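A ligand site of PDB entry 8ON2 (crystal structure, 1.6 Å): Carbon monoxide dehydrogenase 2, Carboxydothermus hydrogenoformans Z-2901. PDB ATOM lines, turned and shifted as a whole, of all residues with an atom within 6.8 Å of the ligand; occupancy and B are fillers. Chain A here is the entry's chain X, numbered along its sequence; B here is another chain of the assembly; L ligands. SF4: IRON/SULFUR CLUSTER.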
ATOM      1  N   CYS A  47     -14.538  -7.085 -11.038  1.00  0.00           N
ATOM      2  CA  CYS A  47     -13.682  -6.905  -9.877  1.00  0.00           C
ATOM      3  C   CYS A  47     -13.262  -8.266  -9.359  1.00  0.00           C
ATOM      4  O   CYS A  47     -14.070  -9.217  -9.329  1.00  0.00           O
ATOM      5  CB  CYS A  47     -14.366  -6.110  -8.774  1.00  0.00           C
ATOM      6  SG  CYS A  47     -13.233  -5.977  -7.344  1.00  0.00           S
ATOM      7  N   CYS A  48     -11.992  -8.357  -8.941  1.00  0.00           N
ATOM      8  CA  CYS A  48     -11.457  -9.616  -8.423  1.00  0.00           C
ATOM      9  C   CYS A  48     -10.580  -9.314  -7.215  1.00  0.00           C
ATOM     10  O   CYS A  48      -9.720  -8.433  -7.258  1.00  0.00           O
ATOM     11  CB  CYS A  48     -10.657 -10.362  -9.491  1.00  0.00           C
ATOM     12  SG  CYS A  48      -9.979 -11.935  -8.900  1.00  0.00           S
ATOM     13  N   ARG A  49     -10.792 -10.099  -6.147  1.00  0.00           N
ATOM     14  CA  ARG A  49      -9.983 -10.025  -4.926  1.00  0.00           C
ATOM     15  C   ARG A  49      -9.512 -11.432  -4.550  1.00  0.00           C
ATOM     16  O   ARG A  49      -9.335 -11.732  -3.365  1.00  0.00           O
ATOM     17  CB  ARG A  49     -10.767  -9.399  -3.788  1.00  0.00           C
ATOM     18  CG  ARG A  49     -11.131  -7.951  -4.078  1.00  0.00           C
ATOM     19  CD  ARG A  49     -12.059  -7.374  -2.989  1.00  0.00           C
ATOM     20  NE  ARG A  49     -11.459  -7.584  -1.695  1.00  0.00           N
ATOM     21  CZ  ARG A  49     -12.093  -8.031  -0.614  1.00  0.00           C
ATOM     22  NH1 ARG A  49     -13.422  -8.135  -0.584  1.00  0.00           N
ATOM     23  NH2 ARG A  49     -11.389  -8.362   0.456  1.00  0.00           N
ATOM     24  N   HIS A  50      -9.312 -12.287  -5.553  1.00  0.00           N
ATOM     25  CA  HIS A  50      -8.950 -13.674  -5.269  1.00  0.00           C
ATOM     26  C   HIS A  50      -7.471 -13.852  -4.931  1.00  0.00           C
ATOM     27  O   HIS A  50      -7.089 -14.969  -4.576  1.00  0.00           O
ATOM     28  CB  HIS A  50      -9.296 -14.598  -6.433  1.00  0.00           C
ATOM     29  CG  HIS A  50     -10.752 -14.785  -6.647  1.00  0.00           C
ATOM     30  ND1 HIS A  50     -11.283 -15.809  -7.407  1.00  0.00           N
ATOM     31  CD2 HIS A  50     -11.812 -14.030  -6.251  1.00  0.00           C
ATOM     32  CE1 HIS A  50     -12.593 -15.695  -7.453  1.00  0.00           C
ATOM     33  NE2 HIS A  50     -12.951 -14.635  -6.745  1.00  0.00           N
ATOM     34  N   CYS A  51      -6.668 -12.787  -4.957  1.00  0.00           N
ATOM     35  CA  CYS A  51      -5.332 -12.880  -4.379  1.00  0.00           C
ATOM     36  C   CYS A  51      -4.907 -11.511  -3.871  1.00  0.00           C
ATOM     37  O   CYS A  51      -5.548 -10.507  -4.139  1.00  0.00           O
ATOM     38  CB  CYS A  51      -4.321 -13.432  -5.370  1.00  0.00           C
ATOM     39  SG  CYS A  51      -3.607 -12.279  -6.526  1.00  0.00           S
ATOM     40  N   LEU A  52      -3.803 -11.502  -3.109  1.00  0.00           N
ATOM     41  CA  LEU A  52      -3.338 -10.291  -2.463  1.00  0.00           C
ATOM     42  C   LEU A  52      -2.552  -9.365  -3.365  1.00  0.00           C
ATOM     43  O   LEU A  52      -2.033  -8.350  -2.885  1.00  0.00           O
ATOM     44  CB  LEU A  52      -2.471 -10.656  -1.253  1.00  0.00           C
ATOM     45  CG  LEU A  52      -3.137 -11.514  -0.184  1.00  0.00           C
ATOM     46  CD1 LEU A  52      -2.134 -11.930   0.845  1.00  0.00           C
ATOM     47  CD2 LEU A  52      -4.269 -10.746   0.476  1.00  0.00           C
ATOM     48  N   GLN A  53      -2.461  -9.658  -4.660  1.00  0.00           N
ATOM     49  CA  GLN A  53      -2.036  -8.651  -5.614  1.00  0.00           C
ATOM     50  C   GLN A  53      -3.170  -7.715  -5.970  1.00  0.00           C
ATOM     51  O   GLN A  53      -2.909  -6.627  -6.481  1.00  0.00           O
ATOM     52  CB  GLN A  53      -1.491  -9.305  -6.880  1.00  0.00           C
ATOM     53  CG  GLN A  53      -0.230 -10.106  -6.611  1.00  0.00           C
ATOM     54  CD  GLN A  53       0.375 -10.774  -7.822  1.00  0.00           C
ATOM     55  OE1 GLN A  53       1.600 -10.864  -7.934  1.00  0.00           O
ATOM     56  NE2 GLN A  53      -0.472 -11.278  -8.724  1.00  0.00           N
ATOM     57  N   GLY A  54      -4.405  -8.145  -5.707  1.00  0.00           N
ATOM     58  CA  GLY A  54      -5.574  -7.341  -5.969  1.00  0.00           C
ATOM     59  C   GLY A  54      -5.744  -6.265  -4.927  1.00  0.00           C
ATOM     60  O   GLY A  54      -4.881  -6.030  -4.074  1.00  0.00           O
ATOM     61  N   PRO A  55      -6.887  -5.579  -4.974  1.00  0.00           N
ATOM     62  CA  PRO A  55      -8.018  -5.809  -5.862  1.00  0.00           C
ATOM     63  C   PRO A  55      -7.684  -5.429  -7.273  1.00  0.00           C
ATOM     64  O   PRO A  55      -6.965  -4.451  -7.542  1.00  0.00           O
ATOM     65  CB  PRO A  55      -9.132  -4.920  -5.251  1.00  0.00           C
ATOM     66  CG  PRO A  55      -8.393  -3.868  -4.471  1.00  0.00           C
ATOM     67  CD  PRO A  55      -7.150  -4.536  -3.978  1.00  0.00           C
ATOM     68  N   CYS A  56      -8.191  -6.215  -8.201  1.00  0.00           N
ATOM     69  CA  CYS A  56      -8.112  -5.926  -9.618  1.00  0.00           C
ATOM     70  C   CYS A  56      -9.490  -5.512 -10.101  1.00  0.00           C
ATOM     71  O   CYS A  56     -10.500  -6.086  -9.701  1.00  0.00           O
ATOM     72  CB  CYS A  56      -7.659  -7.154 -10.397  1.00  0.00           C
ATOM     73  SG  CYS A  56      -5.900  -7.399 -10.111  1.00  0.00           S
ATOM     74  N   ARG A  57      -9.516  -4.511 -10.938  1.00  0.00           N
ATOM     75  CA  ARG A  57     -10.756  -4.148 -11.604  1.00  0.00           C
ATOM     76  C   ARG A  57     -10.461  -4.016 -13.084  1.00  0.00           C
ATOM     77  O   ARG A  57      -9.314  -3.869 -13.503  1.00  0.00           O
ATOM     78  CB  ARG A  57     -11.309  -2.837 -11.048  1.00  0.00           C
ATOM     79  CG  ARG A  57     -10.505  -1.679 -11.537  1.00  0.00           C
ATOM     80  CD  ARG A  57     -10.621  -0.450 -10.666  1.00  0.00           C
ATOM     81  NE  ARG A  57      -9.793   0.612 -11.206  1.00  0.00           N
ATOM     82  CZ  ARG A  57      -8.477   0.719 -11.041  1.00  0.00           C
ATOM     83  NH1 ARG A  57      -7.804  -0.109 -10.239  1.00  0.00           N
ATOM     84  NH2 ARG A  57      -7.818   1.665 -11.710  1.00  0.00           N
ATOM     85  N   VAL A  67      -7.241  -5.771 -17.974  1.00  0.00           N
ATOM     86  CA  VAL A  67      -6.952  -7.163 -17.647  1.00  0.00           C
ATOM     87  C   VAL A  67      -6.443  -7.202 -16.218  1.00  0.00           C
ATOM     88  O   VAL A  67      -5.823  -6.258 -15.743  1.00  0.00           O
ATOM     89  CB  VAL A  67      -5.921  -7.751 -18.652  1.00  0.00           C
ATOM     90  CG1 VAL A  67      -4.605  -7.025 -18.516  1.00  0.00           C
ATOM     91  CG2 VAL A  67      -5.733  -9.215 -18.456  1.00  0.00           C
ATOM     92  N   GLY A  68      -6.739  -8.297 -15.518  1.00  0.00           N
ATOM     93  CA  GLY A  68      -6.230  -8.463 -14.154  1.00  0.00           C
ATOM     94  C   GLY A  68      -4.721  -8.567 -14.121  1.00  0.00           C
ATOM     95  O   GLY A  68      -4.084  -8.842 -15.122  1.00  0.00           O
ATOM     96  N   ILE A  69      -4.142  -8.370 -12.946  1.00  0.00           N
ATOM     97  CA  ILE A  69      -2.686  -8.323 -12.853  1.00  0.00           C
ATOM     98  C   ILE A  69      -2.053  -9.639 -13.262  1.00  0.00           C
ATOM     99  O   ILE A  69      -1.018  -9.660 -13.928  1.00  0.00           O
ATOM    100  CB  ILE A  69      -2.252  -7.887 -11.443  1.00  0.00           C
ATOM    101  CG1 ILE A  69      -2.538  -6.396 -11.226  1.00  0.00           C
ATOM    102  CG2 ILE A  69      -0.781  -8.212 -11.217  1.00  0.00           C
ATOM    103  CD1 ILE A  69      -2.468  -5.970  -9.770  1.00  0.00           C
ATOM    104  N   CYS A  70      -2.688 -10.771 -12.913  1.00  0.00           N
ATOM    105  CA  CYS A  70      -2.155 -12.083 -13.296  1.00  0.00           C
ATOM    106  C   CYS A  70      -2.433 -12.451 -14.754  1.00  0.00           C
ATOM    107  O   CYS A  70      -2.000 -13.521 -15.199  1.00  0.00           O
ATOM    108  CB  CYS A  70      -2.782 -13.164 -12.430  1.00  0.00           C
ATOM    109  SG  CYS A  70      -4.556 -13.232 -12.603  1.00  0.00           S
ATOM    110  N   GLY A  71      -3.165 -11.613 -15.487  1.00  0.00           N
ATOM    111  CA  GLY A  71      -3.583 -11.916 -16.847  1.00  0.00           C
ATOM    112  C   GLY A  71      -5.018 -12.356 -16.990  1.00  0.00           C
ATOM    113  O   GLY A  71      -5.462 -12.614 -18.106  1.00  0.00           O
ATOM    114  N   ALA A  72      -5.756 -12.410 -15.889  1.00  0.00           N
ATOM    115  CA  ALA A  72      -7.144 -12.831 -15.928  1.00  0.00           C
ATOM    116  C   ALA A  72      -7.988 -11.834 -16.727  1.00  0.00           C
ATOM    117  O   ALA A  72      -7.995 -10.638 -16.433  1.00  0.00           O
ATOM    118  CB  ALA A  72      -7.680 -12.999 -14.516  1.00  0.00           C
ATOM    119  N   ILE A  77     -12.668 -13.417 -14.940  1.00  0.00           N
ATOM    120  CA  ILE A  77     -13.031 -12.809 -13.675  1.00  0.00           C
ATOM    121  C   ILE A  77     -14.524 -12.913 -13.430  1.00  0.00           C
ATOM    122  O   ILE A  77     -14.972 -13.244 -12.307  1.00  0.00           O
ATOM    123  CB  ILE A  77     -12.575 -11.342 -13.644  1.00  0.00           C
ATOM    124  CG1 ILE A  77     -11.050 -11.298 -13.491  1.00  0.00           C
ATOM    125  CG2 ILE A  77     -13.225 -10.581 -12.541  1.00  0.00           C
ATOM    126  CD1 ILE A  77     -10.397  -9.963 -13.703  1.00  0.00           C
ATOM    127  N   ARG A  80     -15.482 -16.639 -12.811  1.00  0.00           N
ATOM    128  CA  ARG A  80     -15.003 -17.113 -11.503  1.00  0.00           C
ATOM    129  C   ARG A  80     -15.879 -16.587 -10.388  1.00  0.00           C
ATOM    130  O   ARG A  80     -16.217 -17.322  -9.471  1.00  0.00           O
ATOM    131  CB  ARG A  80     -13.578 -16.685 -11.278  1.00  0.00           C
ATOM    132  CG  ARG A  80     -12.629 -17.452 -12.194  1.00  0.00           C
ATOM    133  CD  ARG A  80     -11.165 -17.249 -11.765  1.00  0.00           C
ATOM    134  NE  ARG A  80     -10.733 -15.870 -11.629  1.00  0.00           N
ATOM    135  CZ  ARG A  80      -9.464 -15.507 -11.579  1.00  0.00           C
ATOM    136  NH1 ARG A  80      -8.489 -16.408 -11.690  1.00  0.00           N
ATOM    137  NH2 ARG A  80      -9.146 -14.224 -11.459  1.00  0.00           N
ATOM    138  N   THR A 197     -11.481 -21.677  -9.127  1.00  0.00           N
ATOM    139  CA  THR A 197     -11.624 -20.246  -9.264  1.00  0.00           C
ATOM    140  C   THR A 197     -10.553 -19.484  -8.502  1.00  0.00           C
ATOM    141  O   THR A 197     -10.516 -18.250  -8.579  1.00  0.00           O
ATOM    142  CB  THR A 197     -13.003 -19.785  -8.744  1.00  0.00           C
ATOM    143  OG1 THR A 197     -13.134 -20.231  -7.409  1.00  0.00           O
ATOM    144  CG2 THR A 197     -14.131 -20.324  -9.635  1.00  0.00           C
ATOM    145  N   SER A 198      -9.704 -20.177  -7.763  1.00  0.00           N
ATOM    146  CA  SER A 198      -8.615 -19.495  -7.078  1.00  0.00           C
ATOM    147  C   SER A 198      -7.548 -19.089  -8.084  1.00  0.00           C
ATOM    148  O   SER A 198      -7.584 -19.427  -9.263  1.00  0.00           O
ATOM    149  CB  SER A 198      -8.051 -20.399  -5.964  1.00  0.00           C
ATOM    150  OG  SER A 198      -7.203 -21.391  -6.498  1.00  0.00           O
ATOM    151  N   MET A 199      -6.623 -18.247  -7.625  1.00  0.00           N
ATOM    152  CA  MET A 199      -5.716 -17.601  -8.579  1.00  0.00           C
ATOM    153  C   MET A 199      -4.903 -18.664  -9.308  1.00  0.00           C
ATOM    154  O   MET A 199      -4.448 -19.654  -8.720  1.00  0.00           O
ATOM    155  CB  MET A 199      -4.796 -16.621  -7.868  1.00  0.00           C
ATOM    156  CG  MET A 199      -3.765 -15.925  -8.780  1.00  0.00           C
ATOM    157  SD  MET A 199      -2.283 -16.922  -8.991  1.00  0.00           S
ATOM    158  CE  MET A 199      -1.428 -15.984 -10.227  1.00  0.00           C
ATOM    159  N   GLY A 200      -4.714 -18.453 -10.612  1.00  0.00           N
ATOM    160  CA  GLY A 200      -3.803 -19.275 -11.372  1.00  0.00           C
ATOM    161  C   GLY A 200      -4.280 -20.663 -11.659  1.00  0.00           C
ATOM    162  O   GLY A 200      -3.465 -21.573 -11.879  1.00  0.00           O
ATOM    163  N   MET B  35      -2.949  -0.994 -13.180  1.00  0.00           N
ATOM    164  CA  MET B  35      -4.027  -1.199 -12.203  1.00  0.00           C
ATOM    165  C   MET B  35      -4.002  -0.147 -11.096  1.00  0.00           C
ATOM    166  O   MET B  35      -4.964  -0.039 -10.331  1.00  0.00           O
ATOM    167  CB  MET B  35      -3.926  -2.605 -11.594  1.00  0.00           C
ATOM    168  CG  MET B  35      -5.148  -3.086 -10.805  1.00  0.00           C
ATOM    169  SD  MET B  35      -6.590  -3.209 -11.895  1.00  0.00           S
ATOM    170  CE  MET B  35      -6.208  -4.570 -12.979  1.00  0.00           C
ATOM    171  N   GLN B  38      -4.920   1.183  -6.856  1.00  0.00           N
ATOM    172  CA  GLN B  38      -5.852   0.104  -6.618  1.00  0.00           C
ATOM    173  C   GLN B  38      -6.916   0.540  -5.617  1.00  0.00           C
ATOM    174  O   GLN B  38      -6.757   1.510  -4.880  1.00  0.00           O
ATOM    175  CB  GLN B  38      -5.130  -1.133  -6.116  1.00  0.00           C
ATOM    176  CG  GLN B  38      -4.387  -1.811  -7.222  1.00  0.00           C
ATOM    177  CD  GLN B  38      -3.603  -2.987  -6.746  1.00  0.00           C
ATOM    178  OE1 GLN B  38      -2.532  -2.828  -6.155  1.00  0.00           O
ATOM    179  NE2 GLN B  38      -4.116  -4.180  -6.998  1.00  0.00           N
ATOM    180  N   PRO B 336      -2.464 -16.724 -16.165  1.00  0.00           N
ATOM    181  CA  PRO B 336      -3.077 -17.037 -17.460  1.00  0.00           C
ATOM    182  C   PRO B 336      -2.511 -16.222 -18.623  1.00  0.00           C
ATOM    183  O   PRO B 336      -2.724 -16.630 -19.774  1.00  0.00           O
ATOM    184  CB  PRO B 336      -4.567 -16.766 -17.240  1.00  0.00           C
ATOM    185  CG  PRO B 336      -4.619 -15.914 -16.002  1.00  0.00           C
ATOM    186  CD  PRO B 336      -3.467 -16.321 -15.147  1.00  0.00           C
ATOM    187  N   MET B 560       0.850 -14.018  -1.629  1.00  0.00           N
ATOM    188  CA  MET B 560      -0.093 -13.653  -2.681  1.00  0.00           C
ATOM    189  C   MET B 560      -1.380 -14.485  -2.678  1.00  0.00           C
ATOM    190  O   MET B 560      -2.479 -13.925  -2.668  1.00  0.00           O
ATOM    191  CB  MET B 560       0.639 -13.777  -4.033  1.00  0.00           C
ATOM    192  CG  MET B 560      -0.151 -13.526  -5.260  1.00  0.00           C
ATOM    193  SD  MET B 560      -0.862 -15.005  -6.009  1.00  0.00           S
ATOM    194  CE  MET B 560       0.583 -15.894  -6.535  1.00  0.00           C
HETATM  195 FE1  SF4 L   1      -5.947  -9.747  -9.637  1.00  0.00          FE
HETATM  196 FE2  SF4 L   1      -7.669 -11.654  -9.178  1.00  0.00          FE
HETATM  197 FE3  SF4 L   1      -5.213 -11.806  -8.098  1.00  0.00          FE
HETATM  198 FE4  SF4 L   1      -5.573 -12.204 -10.761  1.00  0.00          FE
HETATM  199  S1  SF4 L   1      -6.402 -13.523  -9.092  1.00  0.00           S
HETATM  200  S2  SF4 L   1      -4.002 -10.856  -9.751  1.00  0.00           S
HETATM  201  S3  SF4 L   1      -7.236 -10.758 -11.245  1.00  0.00           S
HETATM  202  S4  SF4 L   1      -6.811 -10.284  -7.606  1.00  0.00           S
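SG of Cys 47 sits close to O of Cys 56 (3.6 Å). SG of Cys 48 lies close to N of His 50 (3.4 Å). The side-chain sulfur of Cys 56 lies close to the backbone NH of Ile 69. The guanidinium group of Arg 80 lies close to the side-chain sulfur of Cys 48, at 3.5 Å. The backbone NH of Cys 48 is in hydrogen-bond range of the backbone carbonyl oxygen of Cys 56, at 2.8 Å. The backbone NH (N) of Ala 72 sits close to the side-chain sulfur (SG) of Cys 70, at 3.6 Å. SG of Cys 51 sits close to N of Gln 53 (3.4 Å). O of Gln 53 is in hydrogen-bond range of NE2 of Gln 38 of chain B (2.8 Å).
N of His 50 touches S4 of the ligand (3.8 Å). CA of Gly 68 touches S3 of the ligand, at 3.8 Å. CB of Ile 69 touches S2 of the ligand (3.8 Å). CB of Ala 72 touches S3 of the ligand, 3.99 Å away. Met 199 touches the ligand. Hydrophobic or aromatic side chains that line the ligand: Ile 69, Ala 72 and Met 199. Of the 27 residues printed, 12 come within 4 Å of the ligand. The nearest printed residue that does not touch the ligand is Ile 77 (4.1 Å).
A sulfur (S2) of the ligand lies close to the backbone NH (N) of Cys 70. S4 of the ligand lies close to N of Gly 54, at 3.7 Å. The side-chain amide nitrogen of Gln 53 sits close to a sulfur (S2) of the ligand (3.7 Å). An iron atom (FE3) of the ligand is bound by the side-chain sulfur of Cys 51 (2.3 Å). An iron atom (FE4) of the ligand is bound by the side-chain sulfur of Cys 70, at 2.3 Å. NH2 of Arg 80 sits close to S1 of the ligand. SG of Cys 48 binds FE2 of the ligand (2.3 Å). N of Cys 51 sits close to S4 of the ligand (3.6 Å). The side-chain sulfur of Cys 56 binds an iron atom (FE1) of the ligand, 2.4 Å away.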
